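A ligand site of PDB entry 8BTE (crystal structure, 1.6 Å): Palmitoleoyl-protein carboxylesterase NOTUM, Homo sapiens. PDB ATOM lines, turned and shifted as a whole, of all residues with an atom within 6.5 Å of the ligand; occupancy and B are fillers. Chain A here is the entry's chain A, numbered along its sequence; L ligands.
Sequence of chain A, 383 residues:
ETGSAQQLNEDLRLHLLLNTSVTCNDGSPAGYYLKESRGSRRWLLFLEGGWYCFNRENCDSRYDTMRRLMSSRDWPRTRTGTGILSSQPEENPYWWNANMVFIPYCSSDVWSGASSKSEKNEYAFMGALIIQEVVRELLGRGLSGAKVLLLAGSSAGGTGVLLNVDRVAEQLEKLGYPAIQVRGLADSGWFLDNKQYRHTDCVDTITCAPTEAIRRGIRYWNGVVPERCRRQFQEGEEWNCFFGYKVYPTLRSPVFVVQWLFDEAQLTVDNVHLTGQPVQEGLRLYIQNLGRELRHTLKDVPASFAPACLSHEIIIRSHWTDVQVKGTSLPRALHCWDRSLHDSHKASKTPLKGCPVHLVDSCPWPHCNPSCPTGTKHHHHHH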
ATOM      1  N   GLY A  49      29.137  15.744  -7.303  1.00  0.00           N
ATOM      2  CA  GLY A  49      28.140  14.902  -6.691  1.00  0.00           C
ATOM      3  C   GLY A  49      26.772  15.566  -6.649  1.00  0.00           C
ATOM      4  O   GLY A  49      26.496  16.553  -7.328  1.00  0.00           O
ATOM      5  N   GLY A  50      25.873  14.962  -5.852  1.00  0.00           N
ATOM      6  CA  GLY A  50      24.513  15.465  -5.705  1.00  0.00           C
ATOM      7  C   GLY A  50      23.408  14.411  -5.714  1.00  0.00           C
ATOM      8  O   GLY A  50      22.453  14.504  -6.490  1.00  0.00           O
ATOM      9  N   TRP A  51      23.524  13.416  -4.850  1.00  0.00           N
ATOM     10  CA  TRP A  51      22.546  12.312  -4.699  1.00  0.00           C
ATOM     11  C   TRP A  51      22.329  11.631  -6.057  1.00  0.00           C
ATOM     12  O   TRP A  51      23.304  11.375  -6.789  1.00  0.00           O
ATOM     13  CB  TRP A  51      21.267  12.843  -4.043  1.00  0.00           C
ATOM     14  CG  TRP A  51      21.485  13.161  -2.604  1.00  0.00           C
ATOM     15  CD1 TRP A  51      21.669  14.399  -2.074  1.00  0.00           C
ATOM     16  CD2 TRP A  51      21.569  12.231  -1.514  1.00  0.00           C
ATOM     17  NE1 TRP A  51      21.857  14.299  -0.708  1.00  0.00           N
ATOM     18  CE2 TRP A  51      21.786  12.984  -0.344  1.00  0.00           C
ATOM     19  CE3 TRP A  51      21.464  10.836  -1.417  1.00  0.00           C
ATOM     20  CZ2 TRP A  51      21.919  12.382   0.925  1.00  0.00           C
ATOM     21  CZ3 TRP A  51      21.586  10.237  -0.157  1.00  0.00           C
ATOM     22  CH2 TRP A  51      21.812  11.028   0.994  1.00  0.00           C
ATOM     23  N   TYR A  52      21.093  11.268  -6.383  1.00  0.00           N
ATOM     24  CA  TYR A  52      20.738  10.402  -7.502  1.00  0.00           C
ATOM     25  C   TYR A  52      19.217  10.348  -7.492  1.00  0.00           C
ATOM     26  O   TYR A  52      18.573  10.859  -6.573  1.00  0.00           O
ATOM     27  CB  TYR A  52      21.330   8.986  -7.381  1.00  0.00           C
ATOM     28  CG  TYR A  52      21.240   8.426  -5.968  1.00  0.00           C
ATOM     29  CD1 TYR A  52      20.038   7.936  -5.460  1.00  0.00           C
ATOM     30  CD2 TYR A  52      22.363   8.379  -5.142  1.00  0.00           C
ATOM     31  CE1 TYR A  52      19.956   7.435  -4.167  1.00  0.00           C
ATOM     32  CE2 TYR A  52      22.290   7.881  -3.859  1.00  0.00           C
ATOM     33  CZ  TYR A  52      21.086   7.420  -3.373  1.00  0.00           C
ATOM     34  OH  TYR A  52      21.032   6.921  -2.092  1.00  0.00           O
ATOM     35  N   TYR A 105      27.604  17.041 -12.754  1.00  0.00           N
ATOM     36  CA  TYR A 105      26.800  15.838 -12.559  1.00  0.00           C
ATOM     37  C   TYR A 105      25.383  16.134 -13.027  1.00  0.00           C
ATOM     38  O   TYR A 105      24.654  16.893 -12.366  1.00  0.00           O
ATOM     39  CB  TYR A 105      26.844  15.468 -11.077  1.00  0.00           C
ATOM     40  CG  TYR A 105      26.099  14.242 -10.631  1.00  0.00           C
ATOM     41  CD1 TYR A 105      26.178  13.041 -11.326  1.00  0.00           C
ATOM     42  CD2 TYR A 105      25.385  14.275  -9.429  1.00  0.00           C
ATOM     43  CE1 TYR A 105      25.519  11.899 -10.861  1.00  0.00           C
ATOM     44  CE2 TYR A 105      24.737  13.151  -8.960  1.00  0.00           C
ATOM     45  CZ  TYR A 105      24.794  11.967  -9.668  1.00  0.00           C
ATOM     46  OH  TYR A 105      24.149  10.869  -9.180  1.00  0.00           O
ATOM     47  N   VAL A 110      24.909   8.235 -10.108  1.00  0.00           N
ATOM     48  CA  VAL A 110      26.197   7.972  -9.457  1.00  0.00           C
ATOM     49  C   VAL A 110      27.277   7.684 -10.497  1.00  0.00           C
ATOM     50  O   VAL A 110      28.233   6.930 -10.248  1.00  0.00           O
ATOM     51  CB  VAL A 110      26.079   6.828  -8.416  1.00  0.00           C
ATOM     52  CG1 VAL A 110      27.236   6.889  -7.409  1.00  0.00           C
ATOM     53  CG2 VAL A 110      24.745   6.865  -7.686  1.00  0.00           C
ATOM     54  N   SER A 155      31.253  12.971  -3.000  1.00  0.00           N
ATOM     55  CA  SER A 155      29.911  12.411  -2.733  1.00  0.00           C
ATOM     56  C   SER A 155      29.575  11.409  -3.826  1.00  0.00           C
ATOM     57  O   SER A 155      30.335  10.449  -4.006  1.00  0.00           O
ATOM     58  CB  SER A 155      28.924  13.563  -2.549  1.00  0.00           C
ATOM     59  OG  SER A 155      27.728  13.067  -1.991  1.00  0.00           O
ATOM     60  N   ALA A 156      28.447  11.548  -4.547  1.00  0.00           N
ATOM     61  CA  ALA A 156      28.170  10.648  -5.675  1.00  0.00           C
ATOM     62  C   ALA A 156      29.334  10.642  -6.661  1.00  0.00           C
ATOM     63  O   ALA A 156      29.594   9.614  -7.308  1.00  0.00           O
ATOM     64  CB  ALA A 156      26.858  11.038  -6.387  1.00  0.00           C
ATOM     65  N   GLY A 157      30.042  11.769  -6.797  1.00  0.00           N
ATOM     66  CA  GLY A 157      31.220  11.796  -7.659  1.00  0.00           C
ATOM     67  C   GLY A 157      32.379  10.981  -7.134  1.00  0.00           C
ATOM     68  O   GLY A 157      33.200  10.480  -7.921  1.00  0.00           O
ATOM     69  N   THR A 159      31.986   8.159  -5.320  1.00  0.00           N
ATOM     70  CA  THR A 159      31.642   6.793  -5.716  1.00  0.00           C
ATOM     71  C   THR A 159      31.855   6.626  -7.215  1.00  0.00           C
ATOM     72  O   THR A 159      32.339   5.571  -7.662  1.00  0.00           O
ATOM     73  CB  THR A 159      30.200   6.483  -5.324  1.00  0.00           C
ATOM     74  OG1 THR A 159      29.998   6.779  -3.931  1.00  0.00           O
ATOM     75  CG2 THR A 159      29.891   5.003  -5.571  1.00  0.00           C
ATOM     76  N   SER A 188      34.375  11.312   0.018  1.00  0.00           N
ATOM     77  CA  SER A 188      33.007  11.188   0.570  1.00  0.00           C
ATOM     78  C   SER A 188      32.108  10.289  -0.278  1.00  0.00           C
ATOM     79  O   SER A 188      30.886  10.509  -0.358  1.00  0.00           O
ATOM     80  CB  SER A 188      32.370  12.565   0.770  1.00  0.00           C
ATOM     81  OG  SER A 188      33.195  13.364   1.614  1.00  0.00           O
ATOM     82  N   GLY A 189      32.708   9.253  -0.869  1.00  0.00           N
ATOM     83  CA  GLY A 189      32.003   8.299  -1.683  1.00  0.00           C
ATOM     84  C   GLY A 189      32.164   6.867  -1.202  1.00  0.00           C
ATOM     85  O   GLY A 189      31.899   5.921  -1.966  1.00  0.00           O
ATOM     86  N   PHE A 191      30.810   4.398   1.269  1.00  0.00           N
ATOM     87  CA  PHE A 191      29.653   4.155   2.109  1.00  0.00           C
ATOM     88  C   PHE A 191      29.603   2.713   2.598  1.00  0.00           C
ATOM     89  O   PHE A 191      30.172   1.804   1.979  1.00  0.00           O
ATOM     90  CB  PHE A 191      28.363   4.488   1.343  1.00  0.00           C
ATOM     91  CG  PHE A 191      28.267   5.928   0.986  1.00  0.00           C
ATOM     92  CD1 PHE A 191      27.889   6.853   1.939  1.00  0.00           C
ATOM     93  CD2 PHE A 191      28.654   6.380  -0.283  1.00  0.00           C
ATOM     94  CE1 PHE A 191      27.848   8.209   1.633  1.00  0.00           C
ATOM     95  CE2 PHE A 191      28.581   7.732  -0.598  1.00  0.00           C
ATOM     96  CZ  PHE A 191      28.182   8.647   0.354  1.00  0.00           C
ATOM     97  N   LEU A 192      28.882   2.515   3.702  1.00  0.00           N
ATOM     98  CA  LEU A 192      28.654   1.201   4.285  1.00  0.00           C
ATOM     99  C   LEU A 192      27.208   0.784   4.070  1.00  0.00           C
ATOM    100  O   LEU A 192      26.279   1.558   4.302  1.00  0.00           O
ATOM    101  CB  LEU A 192      28.962   1.207   5.790  1.00  0.00           C
ATOM    102  CG  LEU A 192      30.349   1.721   6.171  1.00  0.00           C
ATOM    103  CD1 LEU A 192      30.517   1.676   7.695  1.00  0.00           C
ATOM    104  CD2 LEU A 192      31.405   0.865   5.484  1.00  0.00           C
ATOM    105  N   ASP A 193      27.015  -0.466   3.643  1.00  0.00           N
ATOM    106  CA  ASP A 193      25.682  -1.050   3.562  1.00  0.00           C
ATOM    107  C   ASP A 193      25.291  -1.635   4.914  1.00  0.00           C
ATOM    108  O   ASP A 193      25.110  -2.841   5.093  1.00  0.00           O
ATOM    109  CB  ASP A 193      25.603  -2.078   2.433  1.00  0.00           C
ATOM    110  CG  ASP A 193      26.731  -3.093   2.480  1.00  0.00           C
ATOM    111  OD1 ASP A 193      27.751  -2.869   3.143  1.00  0.00           O
ATOM    112  OD2 ASP A 193      26.585  -4.139   1.808  1.00  0.00           O
ATOM    113  N   ALA A 209      16.263   2.151   1.478  1.00  0.00           N
ATOM    114  CA  ALA A 209      17.518   2.110   2.229  1.00  0.00           C
ATOM    115  C   ALA A 209      18.715   2.082   1.273  1.00  0.00           C
ATOM    116  O   ALA A 209      18.568   1.862   0.072  1.00  0.00           O
ATOM    117  CB  ALA A 209      17.533   0.874   3.140  1.00  0.00           C
ATOM    118  N   PRO A 210      19.942   2.326   1.804  1.00  0.00           N
ATOM    119  CA  PRO A 210      21.130   2.330   0.945  1.00  0.00           C
ATOM    120  C   PRO A 210      21.540   0.960   0.444  1.00  0.00           C
ATOM    121  O   PRO A 210      22.598   0.464   0.820  1.00  0.00           O
ATOM    122  CB  PRO A 210      22.210   2.908   1.868  1.00  0.00           C
ATOM    123  CG  PRO A 210      21.749   2.584   3.241  1.00  0.00           C
ATOM    124  CD  PRO A 210      20.264   2.767   3.166  1.00  0.00           C
ATOM    125  N   THR A 211      20.710   0.338  -0.394  1.00  0.00           N
ATOM    126  CA  THR A 211      20.951  -0.974  -0.974  1.00  0.00           C
ATOM    127  C   THR A 211      19.877  -1.189  -2.010  1.00  0.00           C
ATOM    128  O   THR A 211      20.166  -1.436  -3.183  1.00  0.00           O
ATOM    129  CB  THR A 211      20.913  -2.101   0.064  1.00  0.00           C
ATOM    130  OG1 THR A 211      20.139  -1.681   1.189  1.00  0.00           O
ATOM    131  CG2 THR A 211      22.305  -2.504   0.509  1.00  0.00           C
ATOM    132  N   ILE A 214      20.070   1.612  -4.753  1.00  0.00           N
ATOM    133  CA  ILE A 214      21.081   1.288  -5.766  1.00  0.00           C
ATOM    134  C   ILE A 214      20.647   0.090  -6.627  1.00  0.00           C
ATOM    135  O   ILE A 214      20.857   0.082  -7.839  1.00  0.00           O
ATOM    136  CB  ILE A 214      22.451   1.026  -5.102  1.00  0.00           C
ATOM    137  CG1 ILE A 214      22.963   2.269  -4.362  1.00  0.00           C
ATOM    138  CG2 ILE A 214      23.478   0.590  -6.132  1.00  0.00           C
ATOM    139  CD1 ILE A 214      23.092   3.476  -5.245  1.00  0.00           C
ATOM    140  N   PHE A 242      28.946  -0.608  -5.792  1.00  0.00           N
ATOM    141  CA  PHE A 242      28.816   0.792  -5.406  1.00  0.00           C
ATOM    142  C   PHE A 242      29.339   1.051  -4.010  1.00  0.00           C
ATOM    143  O   PHE A 242      29.349   2.213  -3.570  1.00  0.00           O
ATOM    144  CB  PHE A 242      27.350   1.252  -5.464  1.00  0.00           C
ATOM    145  CG  PHE A 242      26.841   1.505  -6.850  1.00  0.00           C
ATOM    146  CD1 PHE A 242      26.766   0.465  -7.782  1.00  0.00           C
ATOM    147  CD2 PHE A 242      26.359   2.756  -7.197  1.00  0.00           C
ATOM    148  CE1 PHE A 242      26.260   0.700  -9.048  1.00  0.00           C
ATOM    149  CE2 PHE A 242      25.855   3.000  -8.460  1.00  0.00           C
ATOM    150  CZ  PHE A 242      25.810   1.965  -9.382  1.00  0.00           C
ATOM    151  N   PHE A 243      29.768   0.012  -3.301  1.00  0.00           N
ATOM    152  CA  PHE A 243      30.225   0.156  -1.925  1.00  0.00           C
ATOM    153  C   PHE A 243      31.745   0.042  -1.906  1.00  0.00           C
ATOM    154  O   PHE A 243      32.316  -1.009  -2.223  1.00  0.00           O
ATOM    155  CB  PHE A 243      29.529  -0.864  -1.023  1.00  0.00           C
ATOM    156  CG  PHE A 243      28.104  -0.507  -0.802  1.00  0.00           C
ATOM    157  CD1 PHE A 243      27.746   0.342   0.251  1.00  0.00           C
ATOM    158  CD2 PHE A 243      27.132  -0.898  -1.706  1.00  0.00           C
ATOM    159  CE1 PHE A 243      26.425   0.733   0.408  1.00  0.00           C
ATOM    160  CE2 PHE A 243      25.821  -0.520  -1.544  1.00  0.00           C
ATOM    161  CZ  PHE A 243      25.473   0.316  -0.485  1.00  0.00           C
ATOM    162  N   ASP A 263      30.253  10.438   8.250  1.00  0.00           N
ATOM    163  CA  ASP A 263      29.782  11.166   7.081  1.00  0.00           C
ATOM    164  C   ASP A 263      28.283  11.463   7.206  1.00  0.00           C
ATOM    165  O   ASP A 263      27.474  10.596   7.535  1.00  0.00           O
ATOM    166  CB  ASP A 263      30.077  10.333   5.829  1.00  0.00           C
ATOM    167  CG  ASP A 263      29.726  11.073   4.566  1.00  0.00           C
ATOM    168  OD1 ASP A 263      30.572  11.828   4.058  1.00  0.00           O
ATOM    169  OD2 ASP A 263      28.578  10.891   4.090  1.00  0.00           O
ATOM    170  N   ALA A 265      26.039  12.129   4.928  1.00  0.00           N
ATOM    171  CA  ALA A 265      25.177  11.410   4.008  1.00  0.00           C
ATOM    172  C   ALA A 265      24.992   9.967   4.459  1.00  0.00           C
ATOM    173  O   ALA A 265      23.902   9.399   4.314  1.00  0.00           O
ATOM    174  CB  ALA A 265      25.737  11.468   2.589  1.00  0.00           C
ATOM    175  N   GLN A 266      26.046   9.355   4.998  1.00  0.00           N
ATOM    176  CA  GLN A 266      25.923   8.026   5.607  1.00  0.00           C
ATOM    177  C   GLN A 266      24.899   8.057   6.746  1.00  0.00           C
ATOM    178  O   GLN A 266      24.021   7.187   6.838  1.00  0.00           O
ATOM    179  CB  GLN A 266      27.296   7.551   6.083  1.00  0.00           C
ATOM    180  CG  GLN A 266      27.273   6.195   6.789  1.00  0.00           C
ATOM    181  CD  GLN A 266      27.189   5.034   5.807  1.00  0.00           C
ATOM    182  OE1 GLN A 266      28.015   4.924   4.886  1.00  0.00           O
ATOM    183  NE2 GLN A 266      26.224   4.152   6.021  1.00  0.00           N
ATOM    184  N   VAL A 269      21.237   8.379   5.249  1.00  0.00           N
ATOM    185  CA  VAL A 269      20.674   7.120   4.764  1.00  0.00           C
ATOM    186  C   VAL A 269      20.498   6.120   5.891  1.00  0.00           C
ATOM    187  O   VAL A 269      19.704   5.181   5.759  1.00  0.00           O
ATOM    188  CB  VAL A 269      21.490   6.515   3.615  1.00  0.00           C
ATOM    189  CG1 VAL A 269      21.460   7.434   2.388  1.00  0.00           C
ATOM    190  CG2 VAL A 269      22.911   6.203   4.034  1.00  0.00           C
ATOM    191  N   HIS A 312      30.502  16.385   5.383  1.00  0.00           N
ATOM    192  CA  HIS A 312      30.272  15.761   4.077  1.00  0.00           C
ATOM    193  C   HIS A 312      30.970  16.549   2.982  1.00  0.00           C
ATOM    194  O   HIS A 312      30.700  17.744   2.827  1.00  0.00           O
ATOM    195  CB  HIS A 312      28.781  15.645   3.756  1.00  0.00           C
ATOM    196  CG  HIS A 312      28.498  14.790   2.558  1.00  0.00           C
ATOM    197  ND1 HIS A 312      28.956  13.500   2.449  1.00  0.00           N
ATOM    198  CD2 HIS A 312      27.836  15.060   1.407  1.00  0.00           C
ATOM    199  CE1 HIS A 312      28.575  12.985   1.291  1.00  0.00           C
ATOM    200  NE2 HIS A 312      27.887  13.917   0.638  1.00  0.00           N
HETATM  201  C1  LIG L   1      24.929  12.193  -1.024  1.00  0.00           C
HETATM  202  C2  LIG L   1      25.466  10.461  -2.507  1.00  0.00           C
HETATM  203  C3  LIG L   1      25.929   9.063  -2.801  1.00  0.00           C
HETATM  204  C4  LIG L   1      24.612   8.185  -0.789  1.00  0.00           C
HETATM  205  C5  LIG L   1      24.466   6.818  -0.190  1.00  0.00           C
HETATM  206  C6  LIG L   1      25.295   5.895  -1.075  1.00  0.00           C
HETATM  207  C7  LIG L   1      25.521   4.526  -0.995  1.00  0.00           C
HETATM  208  C8  LIG L   1      26.324   3.844  -1.903  1.00  0.00           C
HETATM  209  C9  LIG L   1      26.904   4.571  -2.953  1.00  0.00           C
HETATM  210  C10 LIG L   1      26.685   5.936  -3.057  1.00  0.00           C
HETATM  211  C11 LIG L   1      25.865   6.600  -2.121  1.00  0.00           C
HETATM  212  N1  LIG L   1      25.468   8.003  -1.949  1.00  0.00           N
HETATM  213  O1  LIG L   1      25.639  11.004  -1.233  1.00  0.00           O
HETATM  214  O2  LIG L   1      24.985  11.073  -3.385  1.00  0.00           O
HETATM  215  O3  LIG L   1      26.631   8.845  -3.724  1.00  0.00           O
HETATM  216 CL1  LIG L   1      24.754   3.742   0.364  1.00  0.00          CL
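O1 of the ligand is in hydrogen-bond range of OG of Ser 155 (3.0 Å). N of Trp 51 lies close to O2 of the ligand (3.1 Å). An oxygen (O3) of the ligand lies close to the backbone NH (N) of Ala 156, 3.4 Å away.
The side-chain hydroxyl of Ser 155 lies within hydrogen-bond range of a ring nitrogen (NE2) of His 312, at 2.8 Å. O of Trp 51 is in hydrogen-bond range of OH of Tyr 105. O of Gly 189 sits at hydrogen-bond distance from OG1 of Thr 159. The side-chain carboxylate (OD2) of Asp 263 lies within hydrogen-bond range of the backbone NH (N) of Ala 265, at 2.9 Å. The side-chain carboxylate (OD1) of Asp 263 lies within hydrogen-bond range of a ring nitrogen (ND1) of His 312, 2.8 Å away.
Tyr 52 touches the ligand (CE2 to N1, 3.7 Å). OG1 of Thr 159 touches C10 of the ligand (3.5 Å). Phe 191 touches the ligand. Pro 210 touches the ligand. Phe 242 touches the ligand. Phe 243 touches the ligand. CB of Ala 265 touches C1 of the ligand, at 3.8 Å. His 312 touches the ligand. 11 residues have an atom within 4 Å of the ligand: Trp 51, Tyr 52, Ser 155, Ala 156, Thr 159, Phe 191, Pro 210, Phe 242, Phe 243, Ala 265 and His 312.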
